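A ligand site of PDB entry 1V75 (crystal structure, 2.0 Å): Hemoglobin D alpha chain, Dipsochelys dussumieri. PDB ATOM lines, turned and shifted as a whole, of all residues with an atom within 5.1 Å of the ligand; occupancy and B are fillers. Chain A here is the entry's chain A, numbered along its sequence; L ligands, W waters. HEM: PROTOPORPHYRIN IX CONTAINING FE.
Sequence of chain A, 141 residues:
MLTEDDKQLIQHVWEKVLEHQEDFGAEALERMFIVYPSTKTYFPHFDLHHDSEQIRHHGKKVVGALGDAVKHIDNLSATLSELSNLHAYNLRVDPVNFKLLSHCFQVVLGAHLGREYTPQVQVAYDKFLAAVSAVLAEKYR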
ATOM      1  N   MET A  32     -29.480 -23.138  -1.888  1.00  0.00           N
ATOM      2  CA  MET A  32     -30.319 -21.971  -2.141  1.00  0.00           C
ATOM      3  C   MET A  32     -29.830 -21.235  -3.394  1.00  0.00           C
ATOM      4  O   MET A  32     -30.617 -20.920  -4.279  1.00  0.00           O
ATOM      5  CB  MET A  32     -30.292 -21.024  -0.940  1.00  0.00           C
ATOM      6  CG  MET A  32     -31.156 -19.769  -1.126  1.00  0.00           C
ATOM      7  SD  MET A  32     -31.072 -18.623   0.255  1.00  0.00           S
ATOM      8  CE  MET A  32     -29.437 -17.893  -0.011  1.00  0.00           C
ATOM      9  N   THR A  39     -31.388 -15.543  -5.315  1.00  0.00           N
ATOM     10  CA  THR A  39     -30.866 -15.230  -3.990  1.00  0.00           C
ATOM     11  C   THR A  39     -29.383 -14.828  -4.024  1.00  0.00           C
ATOM     12  O   THR A  39     -28.889 -14.215  -3.094  1.00  0.00           O
ATOM     13  CB  THR A  39     -31.015 -16.426  -3.033  1.00  0.00           C
ATOM     14  OG1 THR A  39     -30.365 -17.577  -3.596  1.00  0.00           O
ATOM     15  CG2 THR A  39     -32.497 -16.752  -2.809  1.00  0.00           C
ATOM     16  N   TYR A  42     -27.855 -11.085  -3.501  1.00  0.00           N
ATOM     17  CA  TYR A  42     -27.663 -10.530  -2.165  1.00  0.00           C
ATOM     18  C   TYR A  42     -26.192 -10.685  -1.770  1.00  0.00           C
ATOM     19  O   TYR A  42     -25.736 -10.072  -0.805  1.00  0.00           O
ATOM     20  CB  TYR A  42     -28.520 -11.290  -1.141  1.00  0.00           C
ATOM     21  CG  TYR A  42     -29.987 -10.903  -1.132  1.00  0.00           C
ATOM     22  CD1 TYR A  42     -30.425  -9.797  -0.404  1.00  0.00           C
ATOM     23  CD2 TYR A  42     -30.917 -11.623  -1.860  1.00  0.00           C
ATOM     24  CE1 TYR A  42     -31.768  -9.424  -0.413  1.00  0.00           C
ATOM     25  CE2 TYR A  42     -32.266 -11.265  -1.876  1.00  0.00           C
ATOM     26  CZ  TYR A  42     -32.682 -10.160  -1.150  1.00  0.00           C
ATOM     27  OH  TYR A  42     -34.012  -9.812  -1.145  1.00  0.00           O
ATOM     28  N   PHE A  43     -25.472 -11.502  -2.518  1.00  0.00           N
ATOM     29  CA  PHE A  43     -24.064 -11.756  -2.221  1.00  0.00           C
ATOM     30  C   PHE A  43     -23.086 -11.437  -3.362  1.00  0.00           C
ATOM     31  O   PHE A  43     -22.232 -12.251  -3.703  1.00  0.00           O
ATOM     32  CB  PHE A  43     -23.884 -13.226  -1.810  1.00  0.00           C
ATOM     33  CG  PHE A  43     -24.657 -13.604  -0.573  1.00  0.00           C
ATOM     34  CD1 PHE A  43     -26.002 -13.964  -0.662  1.00  0.00           C
ATOM     35  CD2 PHE A  43     -24.035 -13.613   0.674  1.00  0.00           C
ATOM     36  CE1 PHE A  43     -26.713 -14.318   0.484  1.00  0.00           C
ATOM     37  CE2 PHE A  43     -24.745 -13.967   1.820  1.00  0.00           C
ATOM     38  CZ  PHE A  43     -26.082 -14.323   1.730  1.00  0.00           C
ATOM     39  N   HIS A  45     -20.593  -9.526  -3.354  1.00  0.00           N
ATOM     40  CA  HIS A  45     -19.235  -9.414  -2.839  1.00  0.00           C
ATOM     41  C   HIS A  45     -18.616 -10.771  -2.540  1.00  0.00           C
ATOM     42  O   HIS A  45     -17.417 -10.860  -2.288  1.00  0.00           O
ATOM     43  CB  HIS A  45     -19.236  -8.556  -1.567  1.00  0.00           C
ATOM     44  CG  HIS A  45     -20.247  -8.976  -0.547  1.00  0.00           C
ATOM     45  ND1 HIS A  45     -21.582  -9.132  -0.840  1.00  0.00           N
ATOM     46  CD2 HIS A  45     -20.123  -9.206   0.778  1.00  0.00           C
ATOM     47  CE1 HIS A  45     -22.243  -9.438   0.260  1.00  0.00           C
ATOM     48  NE2 HIS A  45     -21.382  -9.490   1.261  1.00  0.00           N
ATOM     49  N   PHE A  46     -19.435 -11.818  -2.578  1.00  0.00           N
ATOM     50  CA  PHE A  46     -18.967 -13.172  -2.318  1.00  0.00           C
ATOM     51  C   PHE A  46     -18.484 -13.928  -3.539  1.00  0.00           C
ATOM     52  O   PHE A  46     -19.033 -13.795  -4.633  1.00  0.00           O
ATOM     53  CB  PHE A  46     -20.091 -14.021  -1.724  1.00  0.00           C
ATOM     54  CG  PHE A  46     -20.210 -13.967  -0.230  1.00  0.00           C
ATOM     55  CD1 PHE A  46     -19.910 -12.801   0.473  1.00  0.00           C
ATOM     56  CD2 PHE A  46     -20.694 -15.064   0.481  1.00  0.00           C
ATOM     57  CE1 PHE A  46     -20.100 -12.731   1.847  1.00  0.00           C
ATOM     58  CE2 PHE A  46     -20.886 -14.997   1.845  1.00  0.00           C
ATOM     59  CZ  PHE A  46     -20.586 -13.833   2.539  1.00  0.00           C
ATOM     60  N   HIS A  57     -17.389 -19.633   5.639  1.00  0.00           N
ATOM     61  CA  HIS A  57     -17.382 -18.756   6.805  1.00  0.00           C
ATOM     62  C   HIS A  57     -18.799 -18.268   7.096  1.00  0.00           C
ATOM     63  O   HIS A  57     -19.211 -18.176   8.259  1.00  0.00           O
ATOM     64  CB  HIS A  57     -16.461 -17.563   6.579  1.00  0.00           C
ATOM     65  CG  HIS A  57     -16.679 -16.443   7.541  1.00  0.00           C
ATOM     66  ND1 HIS A  57     -17.776 -15.603   7.479  1.00  0.00           N
ATOM     67  CD2 HIS A  57     -15.949 -16.022   8.612  1.00  0.00           C
ATOM     68  CE1 HIS A  57     -17.711 -14.729   8.466  1.00  0.00           C
ATOM     69  NE2 HIS A  57     -16.618 -14.959   9.164  1.00  0.00           N
ATOM     70  N   HIS A  58     -19.538 -17.925   6.047  1.00  0.00           N
ATOM     71  CA  HIS A  58     -20.891 -17.446   6.243  1.00  0.00           C
ATOM     72  C   HIS A  58     -21.830 -18.555   6.699  1.00  0.00           C
ATOM     73  O   HIS A  58     -22.688 -18.337   7.548  1.00  0.00           O
ATOM     74  CB  HIS A  58     -21.432 -16.831   4.959  1.00  0.00           C
ATOM     75  CG  HIS A  58     -22.756 -16.163   5.145  1.00  0.00           C
ATOM     76  ND1 HIS A  58     -22.948 -15.131   6.041  1.00  0.00           N
ATOM     77  CD2 HIS A  58     -23.971 -16.436   4.619  1.00  0.00           C
ATOM     78  CE1 HIS A  58     -24.225 -14.802   6.055  1.00  0.00           C
ATOM     79  NE2 HIS A  58     -24.866 -15.578   5.211  1.00  0.00           N
ATOM     80  N   LYS A  61     -21.648 -18.948  10.292  1.00  0.00           N
ATOM     81  CA  LYS A  61     -22.268 -17.838  10.994  1.00  0.00           C
ATOM     82  C   LYS A  61     -23.782 -18.032  11.030  1.00  0.00           C
ATOM     83  O   LYS A  61     -24.427 -17.758  12.045  1.00  0.00           O
ATOM     84  CB  LYS A  61     -21.929 -16.513  10.311  1.00  0.00           C
ATOM     85  CG  LYS A  61     -20.507 -16.004  10.568  1.00  0.00           C
ATOM     86  CD  LYS A  61     -20.374 -15.484  11.988  1.00  0.00           C
ATOM     87  CE  LYS A  61     -19.026 -14.833  12.223  1.00  0.00           C
ATOM     88  NZ  LYS A  61     -18.997 -14.152  13.558  1.00  0.00           N
ATOM     89  N   VAL A  62     -24.352 -18.508   9.926  1.00  0.00           N
ATOM     90  CA  VAL A  62     -25.795 -18.729   9.870  1.00  0.00           C
ATOM     91  C   VAL A  62     -26.172 -19.833  10.869  1.00  0.00           C
ATOM     92  O   VAL A  62     -27.091 -19.671  11.674  1.00  0.00           O
ATOM     93  CB  VAL A  62     -26.250 -19.161   8.450  1.00  0.00           C
ATOM     94  CG1 VAL A  62     -27.745 -19.515   8.465  1.00  0.00           C
ATOM     95  CG2 VAL A  62     -25.982 -18.027   7.464  1.00  0.00           C
ATOM     96  N   ALA A  65     -26.050 -18.556  14.411  1.00  0.00           N
ATOM     97  CA  ALA A  65     -27.215 -17.780  14.828  1.00  0.00           C
ATOM     98  C   ALA A  65     -28.412 -18.690  15.102  1.00  0.00           C
ATOM     99  O   ALA A  65     -29.181 -18.441  16.030  1.00  0.00           O
ATOM    100  CB  ALA A  65     -27.573 -16.765  13.735  1.00  0.00           C
ATOM    101  N   LEU A  66     -28.559 -19.737  14.300  1.00  0.00           N
ATOM    102  CA  LEU A  66     -29.664 -20.665  14.489  1.00  0.00           C
ATOM    103  C   LEU A  66     -29.457 -21.411  15.807  1.00  0.00           C
ATOM    104  O   LEU A  66     -30.413 -21.687  16.538  1.00  0.00           O
ATOM    105  CB  LEU A  66     -29.777 -21.637  13.301  1.00  0.00           C
ATOM    106  CG  LEU A  66     -30.289 -21.003  11.980  1.00  0.00           C
ATOM    107  CD1 LEU A  66     -30.319 -22.037  10.869  1.00  0.00           C
ATOM    108  CD2 LEU A  66     -31.688 -20.432  12.192  1.00  0.00           C
ATOM    109  N   LEU A  83     -29.834  -8.981  14.385  1.00  0.00           N
ATOM    110  CA  LEU A  83     -29.921  -9.618  13.076  1.00  0.00           C
ATOM    111  C   LEU A  83     -31.181  -9.193  12.333  1.00  0.00           C
ATOM    112  O   LEU A  83     -31.196  -9.133  11.094  1.00  0.00           O
ATOM    113  CB  LEU A  83     -29.909 -11.141  13.205  1.00  0.00           C
ATOM    114  CG  LEU A  83     -28.582 -11.698  13.702  1.00  0.00           C
ATOM    115  CD1 LEU A  83     -28.688 -13.214  13.860  1.00  0.00           C
ATOM    116  CD2 LEU A  83     -27.477 -11.330  12.715  1.00  0.00           C
ATOM    117  N   LEU A  86     -30.551  -5.873  10.787  1.00  0.00           N
ATOM    118  CA  LEU A  86     -29.634  -6.053   9.670  1.00  0.00           C
ATOM    119  C   LEU A  86     -30.324  -6.523   8.390  1.00  0.00           C
ATOM    120  O   LEU A  86     -30.166  -5.914   7.334  1.00  0.00           O
ATOM    121  CB  LEU A  86     -28.542  -7.067  10.043  1.00  0.00           C
ATOM    122  CG  LEU A  86     -27.488  -7.344   8.974  1.00  0.00           C
ATOM    123  CD1 LEU A  86     -26.533  -6.161   8.860  1.00  0.00           C
ATOM    124  CD2 LEU A  86     -26.736  -8.598   9.343  1.00  0.00           C
ATOM    125  N   HIS A  87     -31.094  -7.601   8.498  1.00  0.00           N
ATOM    126  CA  HIS A  87     -31.763  -8.153   7.335  1.00  0.00           C
ATOM    127  C   HIS A  87     -32.868  -7.266   6.763  1.00  0.00           C
ATOM    128  O   HIS A  87     -33.122  -7.308   5.555  1.00  0.00           O
ATOM    129  CB  HIS A  87     -32.308  -9.552   7.651  1.00  0.00           C
ATOM    130  CG  HIS A  87     -31.237 -10.592   7.776  1.00  0.00           C
ATOM    131  ND1 HIS A  87     -30.438 -10.689   8.883  1.00  0.00           N
ATOM    132  CD2 HIS A  87     -30.780 -11.515   6.897  1.00  0.00           C
ATOM    133  CE1 HIS A  87     -29.528 -11.632   8.685  1.00  0.00           C
ATOM    134  NE2 HIS A  87     -29.716 -12.141   7.483  1.00  0.00           N
ATOM    135  N   LEU A  91     -29.908  -4.966   4.667  1.00  0.00           N
ATOM    136  CA  LEU A  91     -29.909  -5.849   3.513  1.00  0.00           C
ATOM    137  C   LEU A  91     -31.211  -5.875   2.699  1.00  0.00           C
ATOM    138  O   LEU A  91     -31.212  -6.315   1.549  1.00  0.00           O
ATOM    139  CB  LEU A  91     -29.566  -7.273   3.961  1.00  0.00           C
ATOM    140  CG  LEU A  91     -28.254  -7.414   4.746  1.00  0.00           C
ATOM    141  CD1 LEU A  91     -28.196  -8.773   5.421  1.00  0.00           C
ATOM    142  CD2 LEU A  91     -27.079  -7.216   3.817  1.00  0.00           C
ATOM    143  N   VAL A  93     -33.797  -7.811   2.858  1.00  0.00           N
ATOM    144  CA  VAL A  93     -34.109  -9.162   2.408  1.00  0.00           C
ATOM    145  C   VAL A  93     -35.605  -9.402   2.247  1.00  0.00           C
ATOM    146  O   VAL A  93     -36.390  -9.172   3.170  1.00  0.00           O
ATOM    147  CB  VAL A  93     -33.537 -10.212   3.376  1.00  0.00           C
ATOM    148  CG1 VAL A  93     -33.930 -11.613   2.912  1.00  0.00           C
ATOM    149  CG2 VAL A  93     -32.020 -10.090   3.436  1.00  0.00           C
ATOM    150  N   ASN A  97     -37.430 -15.006   0.749  1.00  0.00           N
ATOM    151  CA  ASN A  97     -36.143 -15.674   0.801  1.00  0.00           C
ATOM    152  C   ASN A  97     -35.837 -16.402   2.097  1.00  0.00           C
ATOM    153  O   ASN A  97     -35.061 -17.360   2.108  1.00  0.00           O
ATOM    154  CB  ASN A  97     -35.041 -14.673   0.456  1.00  0.00           C
ATOM    155  CG  ASN A  97     -35.154 -14.166  -0.966  1.00  0.00           C
ATOM    156  OD1 ASN A  97     -35.433 -14.947  -1.881  1.00  0.00           O
ATOM    157  ND2 ASN A  97     -34.948 -12.877  -1.159  1.00  0.00           N
ATOM    158  N   PHE A  98     -36.447 -15.966   3.199  1.00  0.00           N
ATOM    159  CA  PHE A  98     -36.243 -16.644   4.473  1.00  0.00           C
ATOM    160  C   PHE A  98     -36.856 -18.033   4.352  1.00  0.00           C
ATOM    161  O   PHE A  98     -36.339 -18.999   4.889  1.00  0.00           O
ATOM    162  CB  PHE A  98     -36.892 -15.865   5.612  1.00  0.00           C
ATOM    163  CG  PHE A  98     -36.225 -14.555   5.917  1.00  0.00           C
ATOM    164  CD1 PHE A  98     -34.864 -14.504   6.178  1.00  0.00           C
ATOM    165  CD2 PHE A  98     -36.958 -13.374   5.939  1.00  0.00           C
ATOM    166  CE1 PHE A  98     -34.237 -13.296   6.446  1.00  0.00           C
ATOM    167  CE2 PHE A  98     -36.344 -12.159   6.217  1.00  0.00           C
ATOM    168  CZ  PHE A  98     -34.979 -12.118   6.470  1.00  0.00           C
ATOM    169  N   LEU A 101     -34.450 -20.289   2.230  1.00  0.00           N
ATOM    170  CA  LEU A 101     -33.311 -20.786   2.998  1.00  0.00           C
ATOM    171  C   LEU A 101     -33.750 -21.797   4.056  1.00  0.00           C
ATOM    172  O   LEU A 101     -33.063 -22.790   4.298  1.00  0.00           O
ATOM    173  CB  LEU A 101     -32.547 -19.640   3.666  1.00  0.00           C
ATOM    174  CG  LEU A 101     -31.305 -20.053   4.470  1.00  0.00           C
ATOM    175  CD1 LEU A 101     -30.370 -20.882   3.602  1.00  0.00           C
ATOM    176  CD2 LEU A 101     -30.605 -18.817   4.981  1.00  0.00           C
ATOM    177  N   SER A 102     -34.892 -21.542   4.678  1.00  0.00           N
ATOM    178  CA  SER A 102     -35.420 -22.468   5.685  1.00  0.00           C
ATOM    179  C   SER A 102     -35.639 -23.812   5.021  1.00  0.00           C
ATOM    180  O   SER A 102     -35.274 -24.857   5.566  1.00  0.00           O
ATOM    181  CB  SER A 102     -36.743 -21.958   6.261  1.00  0.00           C
ATOM    182  OG  SER A 102     -36.544 -20.801   7.057  1.00  0.00           O
ATOM    183  N   VAL A 132     -38.122 -18.243  13.437  1.00  0.00           N
ATOM    184  CA  VAL A 132     -36.896 -17.472  13.249  1.00  0.00           C
ATOM    185  C   VAL A 132     -37.077 -16.526  12.063  1.00  0.00           C
ATOM    186  O   VAL A 132     -36.633 -15.370  12.101  1.00  0.00           O
ATOM    187  CB  VAL A 132     -35.692 -18.399  12.951  1.00  0.00           C
ATOM    188  CG1 VAL A 132     -34.436 -17.570  12.698  1.00  0.00           C
ATOM    189  CG2 VAL A 132     -35.454 -19.335  14.110  1.00  0.00           C
ATOM    190  N   LEU A 136     -36.767 -12.371  11.986  1.00  0.00           N
ATOM    191  CA  LEU A 136     -35.818 -11.690  11.113  1.00  0.00           C
ATOM    192  C   LEU A 136     -36.495 -10.733  10.131  1.00  0.00           C
ATOM    193  O   LEU A 136     -35.830  -9.948   9.457  1.00  0.00           O
ATOM    194  CB  LEU A 136     -34.977 -12.701  10.341  1.00  0.00           C
ATOM    195  CG  LEU A 136     -33.914 -13.469  11.150  1.00  0.00           C
ATOM    196  CD1 LEU A 136     -33.278 -14.512  10.259  1.00  0.00           C
ATOM    197  CD2 LEU A 136     -32.863 -12.497  11.663  1.00  0.00           C
HETATM  198  CHA HEM L   1     -25.613 -11.957   7.091  1.00  0.00           C
HETATM  199  CHB HEM L   1     -28.259 -15.028   9.785  1.00  0.00           C
HETATM  200  CHC HEM L   1     -31.309 -15.549   5.987  1.00  0.00           C
HETATM  201  CHD HEM L   1     -28.630 -12.491   3.263  1.00  0.00           C
HETATM  202  C1A HEM L   1     -26.079 -12.727   8.135  1.00  0.00           C
HETATM  203  C2A HEM L   1     -25.418 -12.810   9.435  1.00  0.00           C
HETATM  204  C3A HEM L   1     -26.162 -13.682  10.205  1.00  0.00           C
HETATM  205  C4A HEM L   1     -27.276 -14.134   9.378  1.00  0.00           C
HETATM  206  CMA HEM L   1     -25.891 -14.117  11.629  1.00  0.00           C
HETATM  207  CAA HEM L   1     -24.152 -12.063   9.811  1.00  0.00           C
HETATM  208  CBA HEM L   1     -22.830 -12.831   9.625  1.00  0.00           C
HETATM  209  CGA HEM L   1     -21.639 -12.046  10.173  1.00  0.00           C
HETATM  210  O1A HEM L   1     -21.772 -11.423  11.248  1.00  0.00           O
HETATM  211  O2A HEM L   1     -20.606 -12.093   9.490  1.00  0.00           O
HETATM  212  C1B HEM L   1     -29.310 -15.417   8.971  1.00  0.00           C
HETATM  213  C2B HEM L   1     -30.344 -16.345   9.378  1.00  0.00           C
HETATM  214  C3B HEM L   1     -31.220 -16.498   8.307  1.00  0.00           C
HETATM  215  C4B HEM L   1     -30.702 -15.654   7.235  1.00  0.00           C
HETATM  216  CMB HEM L   1     -30.415 -17.007  10.754  1.00  0.00           C
HETATM  217  CAB HEM L   1     -32.481 -17.355   8.198  1.00  0.00           C
HETATM  218  CBB HEM L   1     -32.299 -18.852   8.358  1.00  0.00           C
HETATM  219  C1C HEM L   1     -30.837 -14.764   4.951  1.00  0.00           C
HETATM  220  C2C HEM L   1     -31.508 -14.705   3.667  1.00  0.00           C
HETATM  221  C3C HEM L   1     -30.741 -13.835   2.895  1.00  0.00           C
HETATM  222  C4C HEM L   1     -29.629 -13.366   3.687  1.00  0.00           C
HETATM  223  CMC HEM L   1     -32.773 -15.470   3.314  1.00  0.00           C
HETATM  224  CAC HEM L   1     -31.025 -13.450   1.461  1.00  0.00           C
HETATM  225  CBC HEM L   1     -30.809 -14.324   0.450  1.00  0.00           C
HETATM  226  C1D HEM L   1     -27.573 -12.086   4.084  1.00  0.00           C
HETATM  227  C2D HEM L   1     -26.504 -11.187   3.679  1.00  0.00           C
HETATM  228  C3D HEM L   1     -25.651 -11.033   4.751  1.00  0.00           C
HETATM  229  C4D HEM L   1     -26.203 -11.847   5.831  1.00  0.00           C
HETATM  230  CMD HEM L   1     -26.338 -10.534   2.327  1.00  0.00           C
HETATM  231  CAD HEM L   1     -24.369 -10.198   4.801  1.00  0.00           C
HETATM  232  CBD HEM L   1     -23.165 -11.102   5.134  1.00  0.00           C
HETATM  233  CGD HEM L   1     -21.794 -10.704   4.629  1.00  0.00           C
HETATM  234  O1D HEM L   1     -21.686  -9.672   3.933  1.00  0.00           O
HETATM  235  O2D HEM L   1     -20.861 -11.466   4.945  1.00  0.00           O
HETATM  236  NA  HEM L   1     -27.160 -13.515   8.160  1.00  0.00           N
HETATM  237  NB  HEM L   1     -29.579 -15.037   7.680  1.00  0.00           N
HETATM  238  NC  HEM L   1     -29.741 -13.959   4.921  1.00  0.00           N
HETATM  239  ND  HEM L   1     -27.325 -12.442   5.381  1.00  0.00           N
HETATM  240 FE   HEM L   1     -28.475 -13.750   6.560  1.00  0.00          FE
HETATM  241  O   HOH W   1     -27.486 -15.398   5.545  1.00  0.00           O
HETATM  242  O   HOH W   2     -18.218 -12.241   4.769  1.00  0.00           O
HETATM  243  O   HOH W   3     -19.323  -8.637   4.433  1.00  0.00           O
HETATM  244  O   HOH W   4     -22.685  -7.302   3.894  1.00  0.00           O
HETATM  245  O   HOH W   5     -20.581 -13.536   6.982  1.00  0.00           O
HETATM  246  O   HOH W   6     -17.904 -11.792   9.923  1.00  0.00           O
HETATM  247  O   HOH W   7     -23.193  -8.941   7.775  1.00  0.00           O
HETATM  248  O   HOH W   8     -23.709 -12.230  13.940  1.00  0.00           O
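A ring nitrogen (ND1) of His 87 lies within hydrogen-bond range of the backbone carbonyl oxygen (O) of Leu 83 (2.8 Å).
The backbone carbonyl oxygen (O) of His 87 is in hydrogen-bond range of the backbone NH (N) of Val 93 (2.8 Å).
The side-chain hydroxyl (OH) of Tyr 42 sits at hydrogen-bond distance from the side-chain amide nitrogen (ND2) of Asn 97 (3.2 Å).
The backbone NH of Leu 91 sits at hydrogen-bond distance from the backbone carbonyl oxygen of Leu 86 (2.8 Å).
OG of Ser 102 is in hydrogen-bond range of O of Phe 98 (2.8 Å).
OG1 of Thr 39 sits close to O of Met 32, 3.4 Å away.
Water W5 lies within hydrogen-bond range of O2A of the ligand (2.9 Å) and ND1 of His 58 (3.0 Å).
Merely in contact with the ligand: Met 32 (3.9 Å), Tyr 42 (3.2 Å), Phe 43 (3.5 Å), Phe 46 (3.4 Å), His 58 (3.3 Å), Lys 61 (3.9 Å), Ala 65 (3.8 Å), Leu 66 (3.9 Å), Leu 83 (3.4 Å), Leu 91 (3.4 Å), Val 93 (3.7 Å), Asn 97 (3.2 Å), Phe 98 (3.7 Å), Leu 101 (3.5 Å) and Leu 136 (3.5 Å).
Hydrophobic or aromatic side chains within 4 Å of the ligand: Met 32, Tyr 42, Phe 43, His 45, Phe 46, His 58, Ala 65, Leu 66, Leu 83, His 87, Leu 91, Val 93, Phe 98, Leu 101 and Leu 136.
Within 4 Å of the ligand: Met 32, Tyr 42, Phe 43, His 45, Phe 46, His 58, Lys 61, Ala 65, Leu 66, Leu 83, His 87, Leu 91, Val 93, Asn 97, Phe 98, Leu 101 and Leu 136.
The nearest printed residue that does not touch the ligand is Thr 39 (4.03 Å).
A ring nitrogen (NE2) of His 87 binds an iron atom (FE) of the ligand (2.2 Å).
O1D of the ligand is in hydrogen-bond range of NE2 of His 45 (2.7 Å).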
